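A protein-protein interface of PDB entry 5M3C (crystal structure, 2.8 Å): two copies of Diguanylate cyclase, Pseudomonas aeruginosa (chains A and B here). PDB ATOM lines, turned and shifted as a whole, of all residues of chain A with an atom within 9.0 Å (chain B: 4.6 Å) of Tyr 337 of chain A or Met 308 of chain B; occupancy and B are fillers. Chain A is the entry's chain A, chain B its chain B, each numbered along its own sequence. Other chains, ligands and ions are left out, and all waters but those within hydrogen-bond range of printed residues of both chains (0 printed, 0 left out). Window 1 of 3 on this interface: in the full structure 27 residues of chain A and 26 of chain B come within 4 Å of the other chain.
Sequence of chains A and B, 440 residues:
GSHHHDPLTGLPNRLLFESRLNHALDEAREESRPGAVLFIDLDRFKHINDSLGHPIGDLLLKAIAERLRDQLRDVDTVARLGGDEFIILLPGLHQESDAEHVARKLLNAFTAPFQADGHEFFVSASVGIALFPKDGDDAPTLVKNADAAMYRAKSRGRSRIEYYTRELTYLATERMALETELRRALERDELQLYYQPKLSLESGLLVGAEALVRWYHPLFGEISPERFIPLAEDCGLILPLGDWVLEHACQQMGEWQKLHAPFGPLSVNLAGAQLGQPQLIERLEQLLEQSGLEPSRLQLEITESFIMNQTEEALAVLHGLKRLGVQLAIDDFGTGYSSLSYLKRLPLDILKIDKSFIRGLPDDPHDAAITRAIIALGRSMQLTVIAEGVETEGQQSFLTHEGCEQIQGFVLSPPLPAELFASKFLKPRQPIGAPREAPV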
ATOM      1  N   LEU A 107      -0.950  -0.001  24.308  1.00  0.00           N
ATOM      2  CA  LEU A 107      -0.766  -1.338  24.862  1.00  0.00           C
ATOM      3  C   LEU A 107      -0.177  -2.288  23.816  1.00  0.00           C
ATOM      4  O   LEU A 107       0.641  -3.145  24.146  1.00  0.00           O
ATOM      5  CB  LEU A 107      -2.095  -1.893  25.380  1.00  0.00           C
ATOM      6  CG  LEU A 107      -2.008  -3.179  26.209  1.00  0.00           C
ATOM      7  CD1 LEU A 107      -1.454  -2.890  27.596  1.00  0.00           C
ATOM      8  CD2 LEU A 107      -3.369  -3.853  26.313  1.00  0.00           C
ATOM      9  N   ASN A 108      -0.589  -2.131  22.559  1.00  0.00           N
ATOM     10  CA  ASN A 108      -0.124  -3.004  21.478  1.00  0.00           C
ATOM     11  C   ASN A 108       1.297  -2.685  21.032  1.00  0.00           C
ATOM     12  O   ASN A 108       1.964  -3.523  20.423  1.00  0.00           O
ATOM     13  CB  ASN A 108      -1.062  -2.929  20.272  1.00  0.00           C
ATOM     14  CG  ASN A 108      -2.205  -3.915  20.369  1.00  0.00           C
ATOM     15  OD1 ASN A 108      -2.561  -4.365  21.459  1.00  0.00           O
ATOM     16  ND2 ASN A 108      -2.785  -4.261  19.227  1.00  0.00           N
ATOM     17  N   PHE A 110       3.619  -2.648  22.868  1.00  0.00           N
ATOM     18  CA  PHE A 110       4.444  -3.519  23.703  1.00  0.00           C
ATOM     19  C   PHE A 110       4.431  -4.988  23.267  1.00  0.00           C
ATOM     20  O   PHE A 110       5.273  -5.771  23.708  1.00  0.00           O
ATOM     21  CB  PHE A 110       3.998  -3.420  25.164  1.00  0.00           C
ATOM     22  CG  PHE A 110       4.287  -2.088  25.799  1.00  0.00           C
ATOM     23  CD1 PHE A 110       5.579  -1.750  26.168  1.00  0.00           C
ATOM     24  CD2 PHE A 110       3.269  -1.181  26.034  1.00  0.00           C
ATOM     25  CE1 PHE A 110       5.851  -0.529  26.754  1.00  0.00           C
ATOM     26  CE2 PHE A 110       3.535   0.042  26.620  1.00  0.00           C
ATOM     27  CZ  PHE A 110       4.827   0.369  26.981  1.00  0.00           C
ATOM     28  N   THR A 111       3.481  -5.364  22.415  1.00  0.00           N
ATOM     29  CA  THR A 111       3.364  -6.751  21.959  1.00  0.00           C
ATOM     30  C   THR A 111       4.614  -7.202  21.212  1.00  0.00           C
ATOM     31  O   THR A 111       5.080  -8.330  21.380  1.00  0.00           O
ATOM     32  CB  THR A 111       2.153  -6.946  21.030  1.00  0.00           C
ATOM     33  OG1 THR A 111       0.945  -6.789  21.781  1.00  0.00           O
ATOM     34  N   ALA A 112       5.149  -6.316  20.380  1.00  0.00           N
ATOM     35  CA  ALA A 112       6.382  -6.591  19.655  1.00  0.00           C
ATOM     36  C   ALA A 112       7.576  -6.505  20.605  1.00  0.00           C
ATOM     37  O   ALA A 112       7.436  -6.035  21.732  1.00  0.00           O
ATOM     38  CB  ALA A 112       6.537  -5.605  18.509  1.00  0.00           C
ATOM     39  N   SER A 159      -0.380  -6.491  31.967  1.00  0.00           N
ATOM     40  CA  SER A 159      -0.377  -6.266  30.530  1.00  0.00           C
ATOM     41  C   SER A 159      -1.791  -5.963  30.037  1.00  0.00           C
ATOM     42  O   SER A 159      -2.277  -6.578  29.087  1.00  0.00           O
ATOM     43  CB  SER A 159       0.188  -7.499  29.819  1.00  0.00           C
ATOM     44  OG  SER A 159      -0.100  -7.472  28.432  1.00  0.00           O
ATOM     45  N   GLU A 304       0.644 -20.487  33.092  1.00  0.00           N
ATOM     46  CA  GLU A 304       1.069 -20.349  31.700  1.00  0.00           C
ATOM     47  C   GLU A 304       1.831 -19.056  31.446  1.00  0.00           C
ATOM     48  O   GLU A 304       2.933 -19.074  30.896  1.00  0.00           O
ATOM     49  CB  GLU A 304      -0.146 -20.403  30.770  1.00  0.00           C
ATOM     50  CG  GLU A 304       0.182 -20.146  29.305  1.00  0.00           C
ATOM     51  CD  GLU A 304      -1.043 -20.186  28.412  1.00  0.00           C
ATOM     52  OE1 GLU A 304      -0.875 -20.365  27.187  1.00  0.00           O
ATOM     53  OE2 GLU A 304      -2.172 -20.043  28.927  1.00  0.00           O
ATOM     54  N   SER A 305       1.233 -17.937  31.848  1.00  0.00           N
ATOM     55  CA  SER A 305       1.777 -16.613  31.547  1.00  0.00           C
ATOM     56  C   SER A 305       3.251 -16.471  31.926  1.00  0.00           C
ATOM     57  O   SER A 305       4.001 -15.760  31.258  1.00  0.00           O
ATOM     58  CB  SER A 305       0.952 -15.527  32.243  1.00  0.00           C
ATOM     59  OG  SER A 305       0.939 -15.718  33.644  1.00  0.00           O
ATOM     60  N   PHE A 306       3.666 -17.143  32.996  1.00  0.00           N
ATOM     61  CA  PHE A 306       5.072 -17.144  33.383  1.00  0.00           C
ATOM     62  C   PHE A 306       5.904 -17.992  32.425  1.00  0.00           C
ATOM     63  O   PHE A 306       6.953 -17.560  31.948  1.00  0.00           O
ATOM     64  CB  PHE A 306       5.250 -17.670  34.805  1.00  0.00           C
ATOM     65  CG  PHE A 306       6.683 -17.930  35.168  1.00  0.00           C
ATOM     66  CD1 PHE A 306       7.264 -19.165  34.914  1.00  0.00           C
ATOM     67  CD2 PHE A 306       7.458 -16.936  35.743  1.00  0.00           C
ATOM     68  CE1 PHE A 306       8.587 -19.406  35.240  1.00  0.00           C
ATOM     69  CE2 PHE A 306       8.782 -17.171  36.070  1.00  0.00           C
ATOM     70  CZ  PHE A 306       9.347 -18.408  35.819  1.00  0.00           C
ATOM     71  N   ILE A 307       5.437 -19.207  32.156  1.00  0.00           N
ATOM     72  CA  ILE A 307       6.165 -20.128  31.295  1.00  0.00           C
ATOM     73  C   ILE A 307       6.331 -19.547  29.901  1.00  0.00           C
ATOM     74  O   ILE A 307       7.358 -19.742  29.260  1.00  0.00           O
ATOM     75  CB  ILE A 307       5.443 -21.481  31.183  1.00  0.00           C
ATOM     76  CG1 ILE A 307       5.629 -22.282  32.470  1.00  0.00           C
ATOM     77  CD1 ILE A 307       5.057 -23.680  32.402  1.00  0.00           C
ATOM     78  N   MET A 308       5.316 -18.822  29.441  1.00  0.00           N
ATOM     79  CA  MET A 308       5.320 -18.254  28.098  1.00  0.00           C
ATOM     80  C   MET A 308       5.686 -16.773  28.123  1.00  0.00           C
ATOM     81  O   MET A 308       4.954 -15.933  27.597  1.00  0.00           O
ATOM     82  CB  MET A 308       3.947 -18.432  27.448  1.00  0.00           C
ATOM     83  CG  MET A 308       3.514 -19.881  27.308  1.00  0.00           C
ATOM     84  SD  MET A 308       4.585 -20.817  26.203  1.00  0.00           S
ATOM     85  CE  MET A 308       3.906 -22.460  26.414  1.00  0.00           C
ATOM     86  N   ASN A 309       6.824 -16.459  28.734  1.00  0.00           N
ATOM     87  CA  ASN A 309       7.309 -15.084  28.766  1.00  0.00           C
ATOM     88  C   ASN A 309       8.353 -14.862  27.675  1.00  0.00           C
ATOM     89  O   ASN A 309       9.248 -14.027  27.818  1.00  0.00           O
ATOM     90  CB  ASN A 309       7.886 -14.745  30.144  1.00  0.00           C
ATOM     91  CG  ASN A 309       9.029 -15.657  30.541  1.00  0.00           C
ATOM     92  OD1 ASN A 309       9.573 -16.391  29.714  1.00  0.00           O
ATOM     93  ND2 ASN A 309       9.398 -15.617  31.815  1.00  0.00           N
ATOM     94  N   GLN A 310       8.229 -15.619  26.586  1.00  0.00           N
ATOM     95  CA  GLN A 310       9.126 -15.499  25.439  1.00  0.00           C
ATOM     96  C   GLN A 310      10.594 -15.623  25.852  1.00  0.00           C
ATOM     97  O   GLN A 310      11.475 -15.032  25.229  1.00  0.00           O
ATOM     98  CB  GLN A 310       8.872 -14.176  24.710  1.00  0.00           C
ATOM     99  CG  GLN A 310       7.393 -13.861  24.528  1.00  0.00           C
ATOM    100  CD  GLN A 310       7.120 -12.889  23.394  1.00  0.00           C
ATOM    101  OE1 GLN A 310       6.607 -11.790  23.612  1.00  0.00           O
ATOM    102  NE2 GLN A 310       7.461 -13.291  22.174  1.00  0.00           N
ATOM    103  N   ILE A 330       0.628 -27.276  33.778  1.00  0.00           N
ATOM    104  CA  ILE A 330       0.540 -25.891  33.327  1.00  0.00           C
ATOM    105  C   ILE A 330      -0.835 -25.337  33.688  1.00  0.00           C
ATOM    106  O   ILE A 330      -1.869 -25.954  33.408  1.00  0.00           O
ATOM    107  CB  ILE A 330       0.833 -25.726  31.818  1.00  0.00           C
ATOM    108  CG1 ILE A 330       0.917 -24.238  31.458  1.00  0.00           C
ATOM    109  CG2 ILE A 330      -0.221 -26.421  30.969  1.00  0.00           C
ATOM    110  CD1 ILE A 330       1.592 -23.961  30.131  1.00  0.00           C
ATOM    111  N   ASP A 332      -3.869 -22.200  34.308  1.00  0.00           N
ATOM    112  CA  ASP A 332      -4.541 -21.063  33.684  1.00  0.00           C
ATOM    113  C   ASP A 332      -4.208 -20.973  32.203  1.00  0.00           C
ATOM    114  O   ASP A 332      -3.765 -19.930  31.722  1.00  0.00           O
ATOM    115  CB  ASP A 332      -4.144 -19.764  34.387  1.00  0.00           C
ATOM    116  CG  ASP A 332      -4.502 -19.768  35.859  1.00  0.00           C
ATOM    117  OD1 ASP A 332      -5.650 -20.128  36.192  1.00  0.00           O
ATOM    118  OD2 ASP A 332      -3.636 -19.409  36.684  1.00  0.00           O
ATOM    119  N   PHE A 333      -4.429 -22.070  31.486  1.00  0.00           N
ATOM    120  CA  PHE A 333      -4.078 -22.137  30.075  1.00  0.00           C
ATOM    121  C   PHE A 333      -5.240 -21.701  29.195  1.00  0.00           C
ATOM    122  O   PHE A 333      -6.410 -21.939  29.524  1.00  0.00           O
ATOM    123  CB  PHE A 333      -3.649 -23.555  29.695  1.00  0.00           C
ATOM    124  CG  PHE A 333      -3.120 -23.669  28.296  1.00  0.00           C
ATOM    125  CD1 PHE A 333      -3.973 -23.925  27.236  1.00  0.00           C
ATOM    126  CD2 PHE A 333      -1.768 -23.514  28.042  1.00  0.00           C
ATOM    127  CE1 PHE A 333      -3.488 -24.026  25.946  1.00  0.00           C
ATOM    128  CE2 PHE A 333      -1.274 -23.615  26.755  1.00  0.00           C
ATOM    129  CZ  PHE A 333      -2.136 -23.871  25.704  1.00  0.00           C
ATOM    130  N   GLY A 334      -4.904 -21.064  28.076  1.00  0.00           N
ATOM    131  CA  GLY A 334      -5.897 -20.647  27.089  1.00  0.00           C
ATOM    132  C   GLY A 334      -5.850 -19.162  26.793  1.00  0.00           C
ATOM    133  O   GLY A 334      -6.187 -18.730  25.693  1.00  0.00           O
ATOM    134  N   THR A 335      -5.432 -18.374  27.776  1.00  0.00           N
ATOM    135  CA  THR A 335      -5.420 -16.926  27.637  1.00  0.00           C
ATOM    136  C   THR A 335      -4.096 -16.445  27.076  1.00  0.00           C
ATOM    137  O   THR A 335      -3.078 -17.126  27.183  1.00  0.00           O
ATOM    138  CB  THR A 335      -5.636 -16.225  28.992  1.00  0.00           C
ATOM    139  OG1 THR A 335      -4.538 -16.519  29.863  1.00  0.00           O
ATOM    140  CG2 THR A 335      -6.937 -16.680  29.637  1.00  0.00           C
ATOM    141  N   GLY A 336      -4.121 -15.260  26.480  1.00  0.00           N
ATOM    142  CA  GLY A 336      -2.905 -14.597  26.039  1.00  0.00           C
ATOM    143  C   GLY A 336      -2.121 -15.372  25.000  1.00  0.00           C
ATOM    144  O   GLY A 336      -2.674 -16.200  24.271  1.00  0.00           O
ATOM    145  N   TYR A 337      -0.820 -15.098  24.941  1.00  0.00           N
ATOM    146  CA  TYR A 337       0.047 -15.660  23.913  1.00  0.00           C
ATOM    147  C   TYR A 337       0.824 -16.860  24.427  1.00  0.00           C
ATOM    148  O   TYR A 337       1.132 -16.953  25.614  1.00  0.00           O
ATOM    149  CB  TYR A 337       1.013 -14.592  23.393  1.00  0.00           C
ATOM    150  CG  TYR A 337       0.349 -13.578  22.493  1.00  0.00           C
ATOM    151  CD1 TYR A 337      -0.562 -12.660  23.004  1.00  0.00           C
ATOM    152  CD2 TYR A 337       0.625 -13.540  21.131  1.00  0.00           C
ATOM    153  CE1 TYR A 337      -1.180 -11.734  22.184  1.00  0.00           C
ATOM    154  CE2 TYR A 337       0.015 -12.616  20.304  1.00  0.00           C
ATOM    155  CZ  TYR A 337      -0.887 -11.716  20.837  1.00  0.00           C
ATOM    156  OH  TYR A 337      -1.498 -10.795  20.020  1.00  0.00           O
ATOM    157  N   SER A 338       1.136 -17.775  23.516  1.00  0.00           N
ATOM    158  CA  SER A 338       1.853 -18.995  23.855  1.00  0.00           C
ATOM    159  C   SER A 338       2.609 -19.527  22.646  1.00  0.00           C
ATOM    160  O   SER A 338       2.364 -19.109  21.514  1.00  0.00           O
ATOM    161  CB  SER A 338       0.875 -20.058  24.359  1.00  0.00           C
ATOM    162  OG  SER A 338      -0.082 -20.385  23.366  1.00  0.00           O
ATOM    163  N   SER A 339       3.530 -20.450  22.898  1.00  0.00           N
ATOM    164  CA  SER A 339       4.317 -21.073  21.841  1.00  0.00           C
ATOM    165  C   SER A 339       4.059 -22.574  21.805  1.00  0.00           C
ATOM    166  O   SER A 339       4.351 -23.283  22.767  1.00  0.00           O
ATOM    167  CB  SER A 339       5.809 -20.809  22.071  1.00  0.00           C
ATOM    168  OG  SER A 339       6.618 -21.611  21.224  1.00  0.00           O
ATOM    169  N   LEU A 340       3.512 -23.053  20.693  1.00  0.00           N
ATOM    170  CA  LEU A 340       3.240 -24.475  20.529  1.00  0.00           C
ATOM    171  C   LEU A 340       4.533 -25.281  20.567  1.00  0.00           C
ATOM    172  O   LEU A 340       4.606 -26.324  21.220  1.00  0.00           O
ATOM    173  CB  LEU A 340       2.501 -24.734  19.216  1.00  0.00           C
ATOM    174  CG  LEU A 340       1.196 -23.957  19.027  1.00  0.00           C
ATOM    175  CD1 LEU A 340       0.412 -24.516  17.851  1.00  0.00           C
ATOM    176  CD2 LEU A 340       0.353 -23.990  20.294  1.00  0.00           C
ATOM    177  N   TYR A 342       7.327 -24.559  22.052  1.00  0.00           N
ATOM    178  CA  TYR A 342       7.842 -24.579  23.414  1.00  0.00           C
ATOM    179  C   TYR A 342       6.940 -25.392  24.333  1.00  0.00           C
ATOM    180  O   TYR A 342       7.408 -25.982  25.304  1.00  0.00           O
ATOM    181  CB  TYR A 342       7.980 -23.151  23.942  1.00  0.00           C
ATOM    182  CG  TYR A 342       8.611 -23.061  25.313  1.00  0.00           C
ATOM    183  CD1 TYR A 342       9.829 -23.673  25.579  1.00  0.00           C
ATOM    184  CD2 TYR A 342       7.997 -22.351  26.337  1.00  0.00           C
ATOM    185  CE1 TYR A 342      10.410 -23.591  26.828  1.00  0.00           C
ATOM    186  CE2 TYR A 342       8.574 -22.261  27.590  1.00  0.00           C
ATOM    187  CZ  TYR A 342       9.781 -22.882  27.829  1.00  0.00           C
ATOM    188  OH  TYR A 342      10.358 -22.796  29.075  1.00  0.00           O
ATOM    189  N   LEU A 343       5.650 -25.421  24.023  1.00  0.00           N
ATOM    190  CA  LEU A 343       4.687 -26.141  24.846  1.00  0.00           C
ATOM    191  C   LEU A 343       4.999 -27.632  24.871  1.00  0.00           C
ATOM    192  O   LEU A 343       4.825 -28.290  25.895  1.00  0.00           O
ATOM    193  CB  LEU A 343       3.265 -25.916  24.329  1.00  0.00           C
ATOM    194  CG  LEU A 343       2.141 -26.404  25.246  1.00  0.00           C
ATOM    195  CD1 LEU A 343       2.093 -25.597  26.535  1.00  0.00           C
ATOM    196  CD2 LEU A 343       0.803 -26.340  24.528  1.00  0.00           C
ATOM    197  N   GLU B 304       1.210 -15.343   9.813  1.00  0.00           N
ATOM    198  CA  GLU B 304       0.852 -15.400  11.230  1.00  0.00           C
ATOM    199  C   GLU B 304       1.494 -14.258  12.008  1.00  0.00           C
ATOM    200  O   GLU B 304       0.802 -13.448  12.634  1.00  0.00           O
ATOM    201  CB  GLU B 304       1.286 -16.742  11.828  1.00  0.00           C
ATOM    202  CG  GLU B 304       0.833 -16.967  13.263  1.00  0.00           C
ATOM    203  CD  GLU B 304       1.433 -18.220  13.876  1.00  0.00           C
ATOM    204  OE1 GLU B 304       0.773 -18.835  14.739  1.00  0.00           O
ATOM    205  OE2 GLU B 304       2.564 -18.593  13.498  1.00  0.00           O
ATOM    206  N   SER B 305       2.821 -14.197  11.949  1.00  0.00           N
ATOM    207  CA  SER B 305       3.597 -13.212  12.700  1.00  0.00           C
ATOM    208  C   SER B 305       2.990 -11.813  12.639  1.00  0.00           C
ATOM    209  O   SER B 305       3.081 -11.050  13.600  1.00  0.00           O
ATOM    210  CB  SER B 305       5.042 -13.176  12.189  1.00  0.00           C
ATOM    211  OG  SER B 305       5.090 -12.986  10.785  1.00  0.00           O
ATOM    212  N   PHE B 306       2.370 -11.480  11.510  1.00  0.00           N
ATOM    213  CA  PHE B 306       1.748 -10.171  11.336  1.00  0.00           C
ATOM    214  C   PHE B 306       0.355 -10.132  11.951  1.00  0.00           C
ATOM    215  O   PHE B 306       0.021  -9.199  12.680  1.00  0.00           O
ATOM    216  CB  PHE B 306       1.653  -9.805   9.854  1.00  0.00           C
ATOM    217  CG  PHE B 306       0.886  -8.542   9.597  1.00  0.00           C
ATOM    218  CD1 PHE B 306      -0.486  -8.575   9.407  1.00  0.00           C
ATOM    219  CD2 PHE B 306       1.531  -7.319   9.561  1.00  0.00           C
ATOM    220  CE1 PHE B 306      -1.198  -7.413   9.179  1.00  0.00           C
ATOM    221  CE2 PHE B 306       0.825  -6.152   9.334  1.00  0.00           C
ATOM    222  CZ  PHE B 306      -0.542  -6.198   9.141  1.00  0.00           C
ATOM    223  N   ILE B 307      -0.455 -11.142  11.649  1.00  0.00           N
ATOM    224  CA  ILE B 307      -1.839 -11.174  12.117  1.00  0.00           C
ATOM    225  C   ILE B 307      -1.932 -11.233  13.641  1.00  0.00           C
ATOM    226  O   ILE B 307      -2.871 -10.695  14.230  1.00  0.00           O
ATOM    227  CB  ILE B 307      -2.621 -12.351  11.498  1.00  0.00           C
ATOM    228  CG1 ILE B 307      -3.367 -11.878  10.249  1.00  0.00           C
ATOM    229  CG2 ILE B 307      -3.614 -12.926  12.496  1.00  0.00           C
ATOM    230  CD1 ILE B 307      -4.405 -12.854   9.735  1.00  0.00           C
ATOM    231  N   MET B 308      -0.960 -11.880  14.277  1.00  0.00           N
ATOM    232  CA  MET B 308      -0.939 -11.966  15.738  1.00  0.00           C
ATOM    233  C   MET B 308      -0.394 -10.684  16.370  1.00  0.00           C
ATOM    234  O   MET B 308      -0.427 -10.518  17.589  1.00  0.00           O
ATOM    235  CB  MET B 308      -0.117 -13.175  16.186  1.00  0.00           C
ATOM    236  CG  MET B 308      -0.747 -14.508  15.811  1.00  0.00           C
ATOM    237  SD  MET B 308      -2.458 -14.656  16.369  1.00  0.00           S
ATOM    238  CE  MET B 308      -2.900 -16.259  15.703  1.00  0.00           C
ATOM    239  N   ASN B 309       0.103  -9.784  15.527  1.00  0.00           N
ATOM    240  CA  ASN B 309       0.556  -8.465  15.958  1.00  0.00           C
ATOM    241  C   ASN B 309      -0.517  -7.418  15.632  1.00  0.00           C
ATOM    242  O   ASN B 309      -0.329  -6.227  15.872  1.00  0.00           O
ATOM    243  CB  ASN B 309       1.872  -8.125  15.250  1.00  0.00           C
ATOM    244  CG  ASN B 309       2.392  -6.742  15.595  1.00  0.00           C
ATOM    245  OD1 ASN B 309       2.549  -6.397  16.768  1.00  0.00           O
ATOM    246  ND2 ASN B 309       2.677  -5.946  14.571  1.00  0.00           N
ATOM    247  N   GLN B 310      -1.647  -7.880  15.099  1.00  0.00           N
ATOM    248  CA  GLN B 310      -2.674  -6.995  14.544  1.00  0.00           C
ATOM    249  C   GLN B 310      -3.418  -6.167  15.593  1.00  0.00           C
ATOM    250  O   GLN B 310      -3.259  -6.374  16.798  1.00  0.00           O
ATOM    251  CB  GLN B 310      -3.684  -7.810  13.728  1.00  0.00           C
ATOM    252  N   TYR B 337       5.284 -17.260  18.935  1.00  0.00           N
ATOM    253  CA  TYR B 337       4.231 -17.075  19.930  1.00  0.00           C
ATOM    254  C   TYR B 337       2.953 -16.552  19.287  1.00  0.00           C
ATOM    255  O   TYR B 337       2.973 -15.549  18.576  1.00  0.00           O
ATOM    256  CB  TYR B 337       4.696 -16.109  21.022  1.00  0.00           C
ATOM    257  CG  TYR B 337       5.594 -16.752  22.050  1.00  0.00           C
ATOM    258  CD1 TYR B 337       6.860 -17.211  21.706  1.00  0.00           C
ATOM    259  CD2 TYR B 337       5.177 -16.904  23.368  1.00  0.00           C
ATOM    260  CE1 TYR B 337       7.686 -17.807  22.645  1.00  0.00           C
ATOM    261  CE2 TYR B 337       5.995 -17.497  24.315  1.00  0.00           C
ATOM    262  CZ  TYR B 337       7.248 -17.949  23.948  1.00  0.00           C
ATOM    263  OH  TYR B 337       8.067 -18.541  24.884  1.00  0.00           O
ATOM    264  N   SER B 338       1.842 -17.233  19.543  1.00  0.00           N
ATOM    265  CA  SER B 338       0.554 -16.841  18.980  1.00  0.00           C
ATOM    266  C   SER B 338      -0.538 -16.907  20.046  1.00  0.00           C
ATOM    267  O   SER B 338      -0.282 -17.305  21.181  1.00  0.00           O
ATOM    268  CB  SER B 338       0.194 -17.744  17.799  1.00  0.00           C
ATOM    269  OG  SER B 338      -0.034 -19.077  18.224  1.00  0.00           O
ATOM    270  N   SER B 339      -1.752 -16.519  19.673  1.00  0.00           N
ATOM    271  CA  SER B 339      -2.872 -16.507  20.607  1.00  0.00           C
ATOM    272  C   SER B 339      -3.997 -17.418  20.134  1.00  0.00           C
ATOM    273  O   SER B 339      -4.607 -17.174  19.094  1.00  0.00           O
ATOM    274  CB  SER B 339      -3.404 -15.083  20.771  1.00  0.00           C
ATOM    275  OG  SER B 339      -4.641 -15.083  21.462  1.00  0.00           O
ATOM    276  N   TYR B 342      -7.333 -15.330  20.011  1.00  0.00           N
ATOM    277  CA  TYR B 342      -7.477 -14.427  18.875  1.00  0.00           C
ATOM    278  C   TYR B 342      -7.613 -15.197  17.559  1.00  0.00           C
ATOM    279  O   TYR B 342      -8.229 -14.715  16.609  1.00  0.00           O
ATOM    280  CB  TYR B 342      -6.267 -13.493  18.825  1.00  0.00           C
ATOM    281  CG  TYR B 342      -6.367 -12.361  17.826  1.00  0.00           C
ATOM    282  CD1 TYR B 342      -7.185 -11.267  18.064  1.00  0.00           C
ATOM    283  CD2 TYR B 342      -5.615 -12.374  16.658  1.00  0.00           C
ATOM    284  CE1 TYR B 342      -7.269 -10.226  17.158  1.00  0.00           C
ATOM    285  CE2 TYR B 342      -5.690 -11.339  15.748  1.00  0.00           C
ATOM    286  CZ  TYR B 342      -6.518 -10.267  16.001  1.00  0.00           C
ATOM    287  OH  TYR B 342      -6.593  -9.232  15.093  1.00  0.00           O
ATOM    288  N   LEU B 343      -7.042 -16.398  17.516  1.00  0.00           N
ATOM    289  CA  LEU B 343      -7.076 -17.235  16.318  1.00  0.00           C
ATOM    290  C   LEU B 343      -8.504 -17.573  15.883  1.00  0.00           C
ATOM    291  O   LEU B 343      -8.784 -17.681  14.690  1.00  0.00           O
ATOM    292  CB  LEU B 343      -6.290 -18.529  16.561  1.00  0.00           C
ATOM    293  CG  LEU B 343      -6.308 -19.580  15.445  1.00  0.00           C
ATOM    294  CD1 LEU B 343      -5.756 -19.010  14.148  1.00  0.00           C
ATOM    295  CD2 LEU B 343      -5.517 -20.810  15.862  1.00  0.00           C
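N of Gln 310 of chain A lies close to OH of Tyr 337 of chain B (3.4 Å).
The side-chain hydroxyl (OH) of Tyr 337 of chain A lies within hydrogen-bond range of the backbone carbonyl oxygen (O) of Met 308 of chain B (2.7 Å).
N of Ser 338 of chain B lies within hydrogen-bond range of O of Ser 338 of chain A, 2.8 Å away.
The side-chain amide nitrogen of Asn 108 of chain A is in hydrogen-bond range of the backbone carbonyl oxygen of Gln 310 of chain B.
The side-chain hydroxyl (OG) of Ser 339 of chain B is in hydrogen-bond range of the backbone NH (N) of Tyr 342 of chain B (3.1 Å).
The backbone NH (N) of Tyr 342 of chain A lies within hydrogen-bond range of the side-chain hydroxyl (OG) of Ser 339 of chain A, at 3.1 Å.
The backbone NH of Ser 339 of chain A sits at hydrogen-bond distance from the side-chain sulfur of Met 308 of chain A.
Among the printed residues, pairs that only touch across the chains: Met 308 of chain A with Tyr 337 of chain B (3.8 Å), Gly 336 of chain A with Ser 339 of chain B (3.6 Å), Tyr 337 of chain A with Ser 338 of chain B (3.2 Å), Ser 338 of chain A with Tyr 337 of chain B (3.2 Å) and Ser 339 of chain A with Tyr 337 of chain B (3.6 Å).
Of the printed residues of chain B, Tyr 337 of chain A touches Met 308 and Ser 338.
Of the printed residues of chain B, Ser 339 of chain A touches Tyr 337.
Met 308 of chain B touches just one residue of chain A: Tyr 337.
Of the printed residues of chain A, Gln 310 of chain B touches Asn 108.
Of the printed residues of chain A, Tyr 337 of chain B touches Met 308 (3.8 Å), Gln 310 (3.3 Å), Ser 338 (3.2 Å) and Ser 339 (3.6 Å).
Ser 338 of chain B touches two residues of chain A.
Printed residues of chain A within 4 Å of Ser 339 of chain B: Gly 336.
The nearest residue of chain A that does not touch Met 308 of chain B is Thr 111 of chain A (5.6 Å).
Hydrophobic or aromatic side chains of chain A that line the printed part of chain B: Met 308 and Tyr 337.
Printed residues of chain B that touch a printed residue of chain A: Met 308, Gln 310, Tyr 337, Ser 338 and Ser 339.
Met 308 of chain A touches Tyr 337 of chain B, and with the chains exchanged Tyr 337 of chain A touches Met 308 of chain B.
Gln 310 of chain A touches Tyr 337 of chain B, but with the chains exchanged Tyr 337 of chain A does not touch Gln 310 of chain B (5.7 Å).
Tyr 337 of chain A touches Ser 338 of chain B, and with the chains exchanged Ser 338 of chain A touches Tyr 337 of chain B.
Ser 338 of chain A touches its own counterpart, Ser 338 of chain B.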
